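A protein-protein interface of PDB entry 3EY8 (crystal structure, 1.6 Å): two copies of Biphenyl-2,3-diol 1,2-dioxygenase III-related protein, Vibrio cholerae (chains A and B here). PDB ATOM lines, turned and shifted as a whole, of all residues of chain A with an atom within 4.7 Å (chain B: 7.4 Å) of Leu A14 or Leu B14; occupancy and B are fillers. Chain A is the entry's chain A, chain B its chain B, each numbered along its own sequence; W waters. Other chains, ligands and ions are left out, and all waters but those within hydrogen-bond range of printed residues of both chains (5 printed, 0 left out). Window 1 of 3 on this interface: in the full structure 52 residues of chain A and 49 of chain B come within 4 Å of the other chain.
NE2 of His A13 is in hydrogen-bond range of OE1 of Glu B126.
O of His A13 lies within hydrogen-bond range of N of Cys B77.
O of Asp A75 is in hydrogen-bond range of N of Val B15, 2.9 Å away.
The side-chain amide oxygen (OE1) of Gln B51 sits at hydrogen-bond distance from the backbone NH (N) of Leu A11, at 3.1 Å.
The backbone NH of Val A15 sits at hydrogen-bond distance from the backbone carbonyl oxygen of Asp B75, 2.9 Å away.
N of Phe B78 lies within hydrogen-bond range of O of Glu B126, at 2.8 Å.
OD2 of Asp B12 lies within hydrogen-bond range of ND1 of His B13 (2.7 Å).
O of Leu B76 lies within hydrogen-bond range of N of Glu B126 (2.8 Å).
O of Leu B14 sits at hydrogen-bond distance from N of Asn B54 (2.9 Å).
O of Leu A14 sits at hydrogen-bond distance from N of Asn A54 (2.8 Å).
The backbone carbonyl oxygen of Leu B11 sits at hydrogen-bond distance from the side-chain amide nitrogen of Gln B51 (2.8 Å).
Among the printed residues, pairs that only touch across the chains: Leu A14 with Asp B75 (3.2 Å), Asp A75 with Leu B14 (3.3 Å), Leu A11 with Cys B77 (3.5 Å), Leu A11 with Phe B48 (3.7 Å), Leu A76 with Leu B14 (3.8 Å), Leu A14 with Leu B76 (3.8 Å), Leu A11 with Leu B14 (3.8 Å), His A13 with Leu B76 (3.8 Å), Leu A76 with His B13 (3.8 Å), Leu A14 with Leu B14 (3.9 Å) and Leu A76 with Leu B11 (3.98 Å).
Leu A14 touches three residues of chain B.
Of the printed residues of chain A, Leu B14 touches Leu A11 (3.8 Å), Leu A14 (3.9 Å), Asp A75 (3.3 Å) and Leu A76 (3.8 Å).
Of the printed residues of chain A, Cys B77 touches Leu A11 and His A13.
Printed residues of chain B within 4 Å of Val A15: Asp B75 (2.9 Å).
Printed residues of chain B within 4 Å of His A13: Leu B76 (3.8 Å), Cys B77 (2.9 Å) and Glu B126 (3.3 Å).
Printed residues of chain A within 4 Å of Asp B75: Leu A14 (3.2 Å) and Val A15 (2.9 Å).
Asn B54 touches none of the printed residues of chain A.
Ala B74 touches none of the printed residues of chain A.
The nearest residue of chain B that does not touch Leu A14 is Leu B11 (4.2 Å).
The nearest printed residue of chain A that does not touch Leu B14 is His A13 (6.8 Å).
Of the 10 printed residues of chain A, 6 touch a printed residue of chain B.
Printed residues of chain A that touch a printed residue of chain B: Leu A11, His A13, Leu A14, Val A15, Asp A75 and Leu A76.
Of the 21 printed residues of chain B, 10 touch a printed residue of chain A.
Printed residues of chain B that touch a printed residue of chain A: Leu B11, His B13, Leu B14, Val B15, Phe B48, Gln B51, Asp B75, Leu B76, Cys B77 and Glu B126.
Among the printed residues, no Asp or Glu carboxylate lies within 4 Å of a Lys or Arg side-chain nitrogen of the other chain.
Leu A11 touches Leu B14, but with the chains exchanged Leu A14 does not touch Leu B11 (4.2 Å).
Leu A14 touches Asp B75, and with the chains exchanged Asp A75 touches Leu B14.
Val A15 touches Asp B75, and with the chains exchanged Asp A75 touches Val B15.
Leu A76 touches Leu B11, but with the chains exchanged Leu A11 does not touch Leu B76 (4.3 Å).
10 positions are printed for both chains.
Of the 16 pairs that touch across the chains among the printed residues, 9 have their exchanged pair printed and touching as well.
Water W5 lies within hydrogen-bond range of the side-chain carboxylate of Glu B126 (2.7 Å) and a ring nitrogen (NE2) of His A13 (3.3 Å).
Water W4 bridges O of Val B15 and N of Asp A75.
Water W2 lies within hydrogen-bond range of N of Asp B75 (2.9 Å) and O of Val A15 (3.1 Å).
Water W3 lies within hydrogen-bond range of OD1 of Asp B75 (2.9 Å), OE1 of Glu B126 (3.3 Å) and NE2 of His A13 (3.4 Å).
Water W1 bridges the side-chain carboxylate (OD1) of Asp A75 (3.0 Å) and a ring nitrogen (NE2) of His B13 (3.4 Å).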
ATOM      1  N   LEU A  11     -11.249 -22.000   7.140  1.00  0.00           N
ATOM      2  CA  LEU A  11     -10.620 -20.697   7.324  1.00  0.00           C
ATOM      3  C   LEU A  11     -10.493 -20.391   8.807  1.00  0.00           C
ATOM      4  O   LEU A  11     -11.493 -20.377   9.531  1.00  0.00           O
ATOM      5  CB  LEU A  11     -11.438 -19.604   6.633  1.00  0.00           C
ATOM      6  CG  LEU A  11     -10.935 -18.168   6.832  1.00  0.00           C
ATOM      7  CD1 LEU A  11     -11.222 -17.339   5.598  1.00  0.00           C
ATOM      8  CD2 LEU A  11     -11.534 -17.523   8.080  1.00  0.00           C
ATOM      9  N   HIS A  13      -8.866 -17.491  10.165  1.00  0.00           N
ATOM     10  CA  HIS A  13      -9.113 -16.083  10.378  1.00  0.00           C
ATOM     11  C   HIS A  13      -8.871 -15.314   9.105  1.00  0.00           C
ATOM     12  O   HIS A  13      -8.445 -15.883   8.092  1.00  0.00           O
ATOM     13  CB  HIS A  13      -8.246 -15.537  11.523  1.00  0.00           C
ATOM     14  CG  HIS A  13      -6.772 -15.629  11.278  1.00  0.00           C
ATOM     15  ND1 HIS A  13      -6.013 -16.695  11.714  1.00  0.00           N
ATOM     16  CD2 HIS A  13      -5.911 -14.777  10.672  1.00  0.00           C
ATOM     17  CE1 HIS A  13      -4.750 -16.500  11.376  1.00  0.00           C
ATOM     18  NE2 HIS A  13      -4.662 -15.344  10.741  1.00  0.00           N
ATOM     19  N   LEU A  14      -9.167 -14.024   9.165  1.00  0.00           N
ATOM     20  CA  LEU A  14      -8.883 -13.108   8.075  1.00  0.00           C
ATOM     21  C   LEU A  14      -8.536 -11.766   8.683  1.00  0.00           C
ATOM     22  O   LEU A  14      -8.810 -11.531   9.860  1.00  0.00           O
ATOM     23  CB  LEU A  14     -10.080 -12.987   7.129  1.00  0.00           C
ATOM     24  CG  LEU A  14     -11.433 -12.517   7.666  1.00  0.00           C
ATOM     25  CD1 LEU A  14     -11.530 -10.995   7.680  1.00  0.00           C
ATOM     26  CD2 LEU A  14     -12.543 -13.106   6.815  1.00  0.00           C
ATOM     27  N   VAL A  15      -7.935 -10.886   7.890  1.00  0.00           N
ATOM     28  CA  VAL A  15      -7.554  -9.568   8.384  1.00  0.00           C
ATOM     29  C   VAL A  15      -8.404  -8.485   7.727  1.00  0.00           C
ATOM     30  O   VAL A  15      -8.483  -8.416   6.496  1.00  0.00           O
ATOM     31  CB  VAL A  15      -6.075  -9.258   8.082  1.00  0.00           C
ATOM     32  CG1 VAL A  15      -5.741  -7.832   8.461  1.00  0.00           C
ATOM     33  CG2 VAL A  15      -5.151 -10.250   8.802  1.00  0.00           C
ATOM     34  N   LEU A  16      -9.038  -7.647   8.544  1.00  0.00           N
ATOM     35  CA  LEU A  16      -9.686  -6.440   8.044  1.00  0.00           C
ATOM     36  C   LEU A  16      -8.802  -5.242   8.345  1.00  0.00           C
ATOM     37  O   LEU A  16      -8.310  -5.099   9.462  1.00  0.00           O
ATOM     38  CB  LEU A  16     -11.037  -6.215   8.721  1.00  0.00           C
ATOM     39  CG  LEU A  16     -12.193  -7.178   8.440  1.00  0.00           C
ATOM     40  CD1 LEU A  16     -13.429  -6.739   9.218  1.00  0.00           C
ATOM     41  CD2 LEU A  16     -12.492  -7.252   6.956  1.00  0.00           C
ATOM     42  N   LYS A  52     -11.540 -16.122  14.144  1.00  0.00           N
ATOM     43  CA  LYS A  52     -11.387 -14.735  14.558  1.00  0.00           C
ATOM     44  C   LYS A  52     -11.163 -13.824  13.358  1.00  0.00           C
ATOM     45  O   LYS A  52     -10.821 -14.280  12.264  1.00  0.00           O
ATOM     46  CB  LYS A  52     -10.242 -14.578  15.568  1.00  0.00           C
ATOM     47  CG  LYS A  52      -8.853 -14.852  14.998  1.00  0.00           C
ATOM     48  CD  LYS A  52      -7.770 -14.405  15.985  1.00  0.00           C
ATOM     49  CE  LYS A  52      -6.372 -14.801  15.516  1.00  0.00           C
ATOM     50  NZ  LYS A  52      -5.339 -13.931  16.143  1.00  0.00           N
ATOM     51  N   ILE A  53     -11.379 -12.533  13.574  1.00  0.00           N
ATOM     52  CA  ILE A  53     -11.008 -11.508  12.605  1.00  0.00           C
ATOM     53  C   ILE A  53      -9.878 -10.673  13.209  1.00  0.00           C
ATOM     54  O   ILE A  53     -10.036 -10.076  14.278  1.00  0.00           O
ATOM     55  CB  ILE A  53     -12.199 -10.592  12.270  1.00  0.00           C
ATOM     56  CG1 ILE A  53     -13.287 -11.390  11.539  1.00  0.00           C
ATOM     57  CG2 ILE A  53     -11.729  -9.396  11.450  1.00  0.00           C
ATOM     58  CD1 ILE A  53     -14.593 -10.638  11.378  1.00  0.00           C
ATOM     59  N   ASN A  54      -8.721 -10.671  12.552  1.00  0.00           N
ATOM     60  CA  ASN A  54      -7.609  -9.827  12.969  1.00  0.00           C
ATOM     61  C   ASN A  54      -7.803  -8.430  12.413  1.00  0.00           C
ATOM     62  O   ASN A  54      -8.208  -8.266  11.260  1.00  0.00           O
ATOM     63  CB  ASN A  54      -6.281 -10.379  12.452  1.00  0.00           C
ATOM     64  CG  ASN A  54      -5.785 -11.569  13.247  1.00  0.00           C
ATOM     65  OD1 ASN A  54      -6.250 -11.837  14.360  1.00  0.00           O
ATOM     66  ND2 ASN A  54      -4.835 -12.290  12.680  1.00  0.00           N
ATOM     67  N   ASP A  75     -16.579  -8.548   2.387  1.00  0.00           N
ATOM     68  CA  ASP A  75     -17.942  -8.938   2.053  1.00  0.00           C
ATOM     69  C   ASP A  75     -18.100 -10.299   2.702  1.00  0.00           C
ATOM     70  O   ASP A  75     -17.633 -11.302   2.170  1.00  0.00           O
ATOM     71  CB  ASP A  75     -18.064  -8.989   0.524  1.00  0.00           C
ATOM     72  CG  ASP A  75     -19.466  -9.314   0.035  1.00  0.00           C
ATOM     73  OD1 ASP A  75     -20.269  -9.895   0.801  1.00  0.00           O
ATOM     74  OD2 ASP A  75     -19.753  -9.000  -1.150  1.00  0.00           O
ATOM     75  N   LEU A  76     -18.730 -10.331   3.873  1.00  0.00           N
ATOM     76  CA  LEU A  76     -18.670 -11.509   4.740  1.00  0.00           C
ATOM     77  C   LEU A  76     -20.040 -12.052   5.079  1.00  0.00           C
ATOM     78  O   LEU A  76     -20.979 -11.283   5.274  1.00  0.00           O
ATOM     79  CB  LEU A  76     -17.963 -11.152   6.054  1.00  0.00           C
ATOM     80  CG  LEU A  76     -16.631 -10.406   5.928  1.00  0.00           C
ATOM     81  CD1 LEU A  76     -16.127 -10.013   7.302  1.00  0.00           C
ATOM     82  CD2 LEU A  76     -15.606 -11.252   5.167  1.00  0.00           C
ATOM     83  N   LEU B  11     -18.015 -18.236  10.281  1.00  0.00           N
ATOM     84  CA  LEU B  11     -18.088 -17.592   8.981  1.00  0.00           C
ATOM     85  C   LEU B  11     -18.487 -18.624   7.936  1.00  0.00           C
ATOM     86  O   LEU B  11     -17.823 -19.650   7.784  1.00  0.00           O
ATOM     87  CB  LEU B  11     -16.740 -16.968   8.609  1.00  0.00           C
ATOM     88  CG  LEU B  11     -16.705 -16.279   7.235  1.00  0.00           C
ATOM     89  CD1 LEU B  11     -17.246 -14.852   7.322  1.00  0.00           C
ATOM     90  CD2 LEU B  11     -15.300 -16.272   6.652  1.00  0.00           C
ATOM     91  N   ASP B  12     -19.570 -18.364   7.216  1.00  0.00           N
ATOM     92  CA  ASP B  12     -20.030 -19.311   6.207  1.00  0.00           C
ATOM     93  C   ASP B  12     -19.266 -19.151   4.899  1.00  0.00           C
ATOM     94  O   ASP B  12     -18.855 -20.126   4.269  1.00  0.00           O
ATOM     95  CB  ASP B  12     -21.522 -19.150   5.937  1.00  0.00           C
ATOM     96  CG  ASP B  12     -22.044 -20.199   4.972  1.00  0.00           C
ATOM     97  OD1 ASP B  12     -22.307 -21.326   5.426  1.00  0.00           O
ATOM     98  OD2 ASP B  12     -22.183 -19.899   3.769  1.00  0.00           O
ATOM     99  N   HIS B  13     -19.090 -17.908   4.482  1.00  0.00           N
ATOM    100  CA  HIS B  13     -18.335 -17.631   3.276  1.00  0.00           C
ATOM    101  C   HIS B  13     -17.947 -16.168   3.226  1.00  0.00           C
ATOM    102  O   HIS B  13     -18.376 -15.370   4.075  1.00  0.00           O
ATOM    103  CB  HIS B  13     -19.123 -18.037   2.019  1.00  0.00           C
ATOM    104  CG  HIS B  13     -20.411 -17.294   1.818  1.00  0.00           C
ATOM    105  ND1 HIS B  13     -21.615 -17.734   2.336  1.00  0.00           N
ATOM    106  CD2 HIS B  13     -20.694 -16.170   1.116  1.00  0.00           C
ATOM    107  CE1 HIS B  13     -22.576 -16.902   1.976  1.00  0.00           C
ATOM    108  NE2 HIS B  13     -22.046 -15.945   1.236  1.00  0.00           N
ATOM    109  N   LEU B  14     -17.118 -15.825   2.243  1.00  0.00           N
ATOM    110  CA  LEU B  14     -16.763 -14.442   1.973  1.00  0.00           C
ATOM    111  C   LEU B  14     -16.685 -14.271   0.463  1.00  0.00           C
ATOM    112  O   LEU B  14     -16.660 -15.259  -0.271  1.00  0.00           O
ATOM    113  CB  LEU B  14     -15.436 -14.069   2.641  1.00  0.00           C
ATOM    114  CG  LEU B  14     -14.196 -14.861   2.226  1.00  0.00           C
ATOM    115  CD1 LEU B  14     -13.512 -14.220   1.026  1.00  0.00           C
ATOM    116  CD2 LEU B  14     -13.229 -14.943   3.404  1.00  0.00           C
ATOM    117  N   VAL B  15     -16.651 -13.028  -0.004  1.00  0.00           N
ATOM    118  CA  VAL B  15     -16.622 -12.768  -1.435  1.00  0.00           C
ATOM    119  C   VAL B  15     -15.292 -12.126  -1.810  1.00  0.00           C
ATOM    120  O   VAL B  15     -14.863 -11.165  -1.172  1.00  0.00           O
ATOM    121  CB  VAL B  15     -17.756 -11.812  -1.859  1.00  0.00           C
ATOM    122  CG1 VAL B  15     -17.596 -11.430  -3.335  1.00  0.00           C
ATOM    123  CG2 VAL B  15     -19.123 -12.428  -1.585  1.00  0.00           C
ATOM    124  N   LEU B  16     -14.627 -12.680  -2.819  1.00  0.00           N
ATOM    125  CA  LEU B  16     -13.456 -12.043  -3.411  1.00  0.00           C
ATOM    126  C   LEU B  16     -13.848 -11.520  -4.778  1.00  0.00           C
ATOM    127  O   LEU B  16     -14.499 -12.221  -5.555  1.00  0.00           O
ATOM    128  CB  LEU B  16     -12.319 -13.039  -3.604  1.00  0.00           C
ATOM    129  CG  LEU B  16     -11.691 -13.680  -2.371  1.00  0.00           C
ATOM    130  CD1 LEU B  16     -10.582 -14.611  -2.829  1.00  0.00           C
ATOM    131  CD2 LEU B  16     -11.163 -12.622  -1.418  1.00  0.00           C
ATOM    132  N   THR B  17     -13.438 -10.291  -5.062  1.00  0.00           N
ATOM    133  CA  THR B  17     -13.579  -9.722  -6.390  1.00  0.00           C
ATOM    134  C   THR B  17     -12.233  -9.852  -7.093  1.00  0.00           C
ATOM    135  O   THR B  17     -11.204  -9.410  -6.572  1.00  0.00           O
ATOM    136  CB  THR B  17     -14.039  -8.268  -6.323  1.00  0.00           C
ATOM    137  OG1 THR B  17     -15.274  -8.206  -5.590  1.00  0.00           O
ATOM    138  CG2 THR B  17     -14.258  -7.710  -7.738  1.00  0.00           C
ATOM    139  N   ALA B  45     -17.967 -20.338  -7.219  1.00  0.00           N
ATOM    140  CA  ALA B  45     -17.440 -20.392  -5.861  1.00  0.00           C
ATOM    141  C   ALA B  45     -16.335 -21.434  -5.727  1.00  0.00           C
ATOM    142  O   ALA B  45     -16.201 -22.331  -6.560  1.00  0.00           O
ATOM    143  CB  ALA B  45     -18.550 -20.673  -4.872  1.00  0.00           C
ATOM    144  N   LEU B  46     -15.545 -21.293  -4.669  1.00  0.00           N
ATOM    145  CA  LEU B  46     -14.527 -22.271  -4.300  1.00  0.00           C
ATOM    146  C   LEU B  46     -14.881 -22.916  -2.964  1.00  0.00           C
ATOM    147  O   LEU B  46     -15.023 -22.222  -1.954  1.00  0.00           O
ATOM    148  CB  LEU B  46     -13.168 -21.584  -4.184  1.00  0.00           C
ATOM    149  CG  LEU B  46     -12.550 -21.129  -5.504  1.00  0.00           C
ATOM    150  CD1 LEU B  46     -11.507 -20.045  -5.265  1.00  0.00           C
ATOM    151  CD2 LEU B  46     -11.948 -22.305  -6.237  1.00  0.00           C
ATOM    152  N   PHE B  48     -14.253 -25.539   0.307  1.00  0.00           N
ATOM    153  CA  PHE B  48     -13.253 -26.196   1.142  1.00  0.00           C
ATOM    154  C   PHE B  48     -13.927 -26.515   2.465  1.00  0.00           C
ATOM    155  O   PHE B  48     -14.650 -25.681   2.998  1.00  0.00           O
ATOM    156  CB  PHE B  48     -12.034 -25.292   1.354  1.00  0.00           C
ATOM    157  CG  PHE B  48     -12.375 -23.918   1.871  1.00  0.00           C
ATOM    158  CD1 PHE B  48     -12.755 -22.908   1.000  1.00  0.00           C
ATOM    159  CD2 PHE B  48     -12.300 -23.633   3.226  1.00  0.00           C
ATOM    160  CE1 PHE B  48     -13.072 -21.647   1.469  1.00  0.00           C
ATOM    161  CE2 PHE B  48     -12.620 -22.365   3.707  1.00  0.00           C
ATOM    162  CZ  PHE B  48     -13.004 -21.376   2.824  1.00  0.00           C
ATOM    163  N   GLN B  51     -17.187 -24.688   4.080  1.00  0.00           N
ATOM    164  CA  GLN B  51     -17.295 -23.265   3.803  1.00  0.00           C
ATOM    165  C   GLN B  51     -17.006 -23.038   2.324  1.00  0.00           C
ATOM    166  O   GLN B  51     -16.731 -23.990   1.591  1.00  0.00           O
ATOM    167  CB  GLN B  51     -16.326 -22.481   4.701  1.00  0.00           C
ATOM    168  CG  GLN B  51     -16.553 -22.746   6.203  1.00  0.00           C
ATOM    169  CD  GLN B  51     -15.477 -22.159   7.124  1.00  0.00           C
ATOM    170  OE1 GLN B  51     -14.281 -22.190   6.824  1.00  0.00           O
ATOM    171  NE2 GLN B  51     -15.910 -21.647   8.272  1.00  0.00           N
ATOM    172  N   LYS B  52     -17.090 -21.793   1.873  1.00  0.00           N
ATOM    173  CA  LYS B  52     -16.745 -21.476   0.494  1.00  0.00           C
ATOM    174  C   LYS B  52     -16.316 -20.028   0.367  1.00  0.00           C
ATOM    175  O   LYS B  52     -16.519 -19.223   1.277  1.00  0.00           O
ATOM    176  CB  LYS B  52     -17.929 -21.728  -0.436  1.00  0.00           C
ATOM    177  CG  LYS B  52     -19.079 -20.728  -0.270  1.00  0.00           C
ATOM    178  CD  LYS B  52     -20.112 -20.918  -1.375  1.00  0.00           C
ATOM    179  CE  LYS B  52     -21.341 -20.048  -1.159  1.00  0.00           C
ATOM    180  NZ  LYS B  52     -22.137 -19.938  -2.418  1.00  0.00           N
ATOM    181  N   ILE B  53     -15.707 -19.712  -0.770  1.00  0.00           N
ATOM    182  CA  ILE B  53     -15.453 -18.335  -1.147  1.00  0.00           C
ATOM    183  C   ILE B  53     -16.186 -18.074  -2.455  1.00  0.00           C
ATOM    184  O   ILE B  53     -16.002 -18.806  -3.429  1.00  0.00           O
ATOM    185  CB  ILE B  53     -13.954 -18.105  -1.328  1.00  0.00           C
ATOM    186  CG1 ILE B  53     -13.253 -18.164   0.029  1.00  0.00           C
ATOM    187  CG2 ILE B  53     -13.697 -16.775  -2.027  1.00  0.00           C
ATOM    188  CD1 ILE B  53     -11.758 -18.315  -0.070  1.00  0.00           C
ATOM    189  N   ASN B  54     -17.053 -17.067  -2.469  1.00  0.00           N
ATOM    190  CA  ASN B  54     -17.730 -16.671  -3.698  1.00  0.00           C
ATOM    191  C   ASN B  54     -16.810 -15.763  -4.496  1.00  0.00           C
ATOM    192  O   ASN B  54     -16.108 -14.921  -3.928  1.00  0.00           O
ATOM    193  CB  ASN B  54     -19.038 -15.930  -3.400  1.00  0.00           C
ATOM    194  CG  ASN B  54     -20.169 -16.861  -2.954  1.00  0.00           C
ATOM    195  OD1 ASN B  54     -20.160 -18.065  -3.236  1.00  0.00           O
ATOM    196  ND2 ASN B  54     -21.157 -16.294  -2.266  1.00  0.00           N
ATOM    197  N   LEU B  55     -16.806 -15.935  -5.811  1.00  0.00           N
ATOM    198  CA  LEU B  55     -15.986 -15.096  -6.674  1.00  0.00           C
ATOM    199  C   LEU B  55     -16.864 -14.180  -7.520  1.00  0.00           C
ATOM    200  O   LEU B  55     -17.823 -14.645  -8.139  1.00  0.00           O
ATOM    201  CB  LEU B  55     -15.123 -15.962  -7.595  1.00  0.00           C
ATOM    202  CG  LEU B  55     -14.138 -16.900  -6.894  1.00  0.00           C
ATOM    203  CD1 LEU B  55     -13.396 -17.775  -7.904  1.00  0.00           C
ATOM    204  CD2 LEU B  55     -13.158 -16.104  -6.026  1.00  0.00           C
ATOM    205  N   ALA B  74      -7.741  -8.859   0.101  1.00  0.00           N
ATOM    206  CA  ALA B  74      -8.020  -9.881   1.110  1.00  0.00           C
ATOM    207  C   ALA B  74      -6.750 -10.453   1.725  1.00  0.00           C
ATOM    208  O   ALA B  74      -5.685 -10.446   1.112  1.00  0.00           O
ATOM    209  CB  ALA B  74      -8.874 -10.992   0.518  1.00  0.00           C
ATOM    210  N   ASP B  75      -6.896 -10.974   2.937  1.00  0.00           N
ATOM    211  CA  ASP B  75      -5.779 -11.427   3.745  1.00  0.00           C
ATOM    212  C   ASP B  75      -6.382 -12.558   4.566  1.00  0.00           C
ATOM    213  O   ASP B  75      -7.103 -12.309   5.538  1.00  0.00           O
ATOM    214  CB  ASP B  75      -5.313 -10.251   4.607  1.00  0.00           C
ATOM    215  CG  ASP B  75      -4.094 -10.564   5.467  1.00  0.00           C
ATOM    216  OD1 ASP B  75      -3.826 -11.742   5.771  1.00  0.00           O
ATOM    217  OD2 ASP B  75      -3.418  -9.594   5.873  1.00  0.00           O
ATOM    218  N   LEU B  76      -6.117 -13.798   4.142  1.00  0.00           N
ATOM    219  CA  LEU B  76      -6.860 -14.969   4.624  1.00  0.00           C
ATOM    220  C   LEU B  76      -5.947 -16.056   5.175  1.00  0.00           C
ATOM    221  O   LEU B  76      -4.874 -16.309   4.626  1.00  0.00           O
ATOM    222  CB  LEU B  76      -7.661 -15.566   3.469  1.00  0.00           C
ATOM    223  CG  LEU B  76      -8.479 -14.598   2.617  1.00  0.00           C
ATOM    224  CD1 LEU B  76      -9.079 -15.323   1.421  1.00  0.00           C
ATOM    225  CD2 LEU B  76      -9.564 -13.958   3.473  1.00  0.00           C
ATOM    226  N   CYS B  77      -6.384 -16.716   6.248  1.00  0.00           N
ATOM    227  CA  CYS B  77      -5.599 -17.799   6.828  1.00  0.00           C
ATOM    228  C   CYS B  77      -6.385 -19.099   6.805  1.00  0.00           C
ATOM    229  O   CYS B  77      -7.451 -19.196   7.409  1.00  0.00           O
ATOM    230  CB  CYS B  77      -5.165 -17.475   8.260  1.00  0.00           C
ATOM    231  SG  CYS B  77      -4.408 -18.908   9.094  1.00  0.00           S
ATOM    232  N   PHE B  78      -5.848 -20.084   6.097  1.00  0.00           N
ATOM    233  CA  PHE B  78      -6.485 -21.394   5.949  1.00  0.00           C
ATOM    234  C   PHE B  78      -5.702 -22.454   6.703  1.00  0.00           C
ATOM    235  O   PHE B  78      -4.476 -22.498   6.624  1.00  0.00           O
ATOM    236  CB  PHE B  78      -6.503 -21.810   4.478  1.00  0.00           C
ATOM    237  CG  PHE B  78      -7.299 -20.896   3.596  1.00  0.00           C
ATOM    238  CD1 PHE B  78      -6.663 -20.078   2.674  1.00  0.00           C
ATOM    239  CD2 PHE B  78      -8.678 -20.860   3.683  1.00  0.00           C
ATOM    240  CE1 PHE B  78      -7.392 -19.232   1.848  1.00  0.00           C
ATOM    241  CE2 PHE B  78      -9.415 -20.015   2.862  1.00  0.00           C
ATOM    242  CZ  PHE B  78      -8.765 -19.202   1.946  1.00  0.00           C
ATOM    243  N   GLU B 126      -2.287 -17.180   3.835  1.00  0.00           N
ATOM    244  CA  GLU B 126      -1.520 -17.754   4.923  1.00  0.00           C
ATOM    245  C   GLU B 126      -2.036 -19.170   5.110  1.00  0.00           C
ATOM    246  O   GLU B 126      -3.213 -19.370   5.396  1.00  0.00           O
ATOM    247  CB  GLU B 126      -1.752 -16.926   6.196  1.00  0.00           C
ATOM    248  CG  GLU B 126      -0.954 -17.375   7.414  1.00  0.00           C
ATOM    249  CD  GLU B 126      -1.300 -16.566   8.651  1.00  0.00           C
ATOM    250  OE1 GLU B 126      -2.178 -15.677   8.563  1.00  0.00           O
ATOM    251  OE2 GLU B 126      -0.699 -16.822   9.713  1.00  0.00           O
HETATM  252  O   HOH W   1     -21.099 -12.642   1.494  1.00  0.00           O
HETATM  253  O   HOH W   2      -9.420 -10.215   4.213  1.00  0.00           O
HETATM  254  O   HOH W   3      -4.696 -13.820   7.654  1.00  0.00           O
HETATM  255  O   HOH W   4     -14.341 -10.371   1.591  1.00  0.00           O
HETATM  256  O   HOH W   5      -1.482 -14.820  11.369  1.00  0.00           O
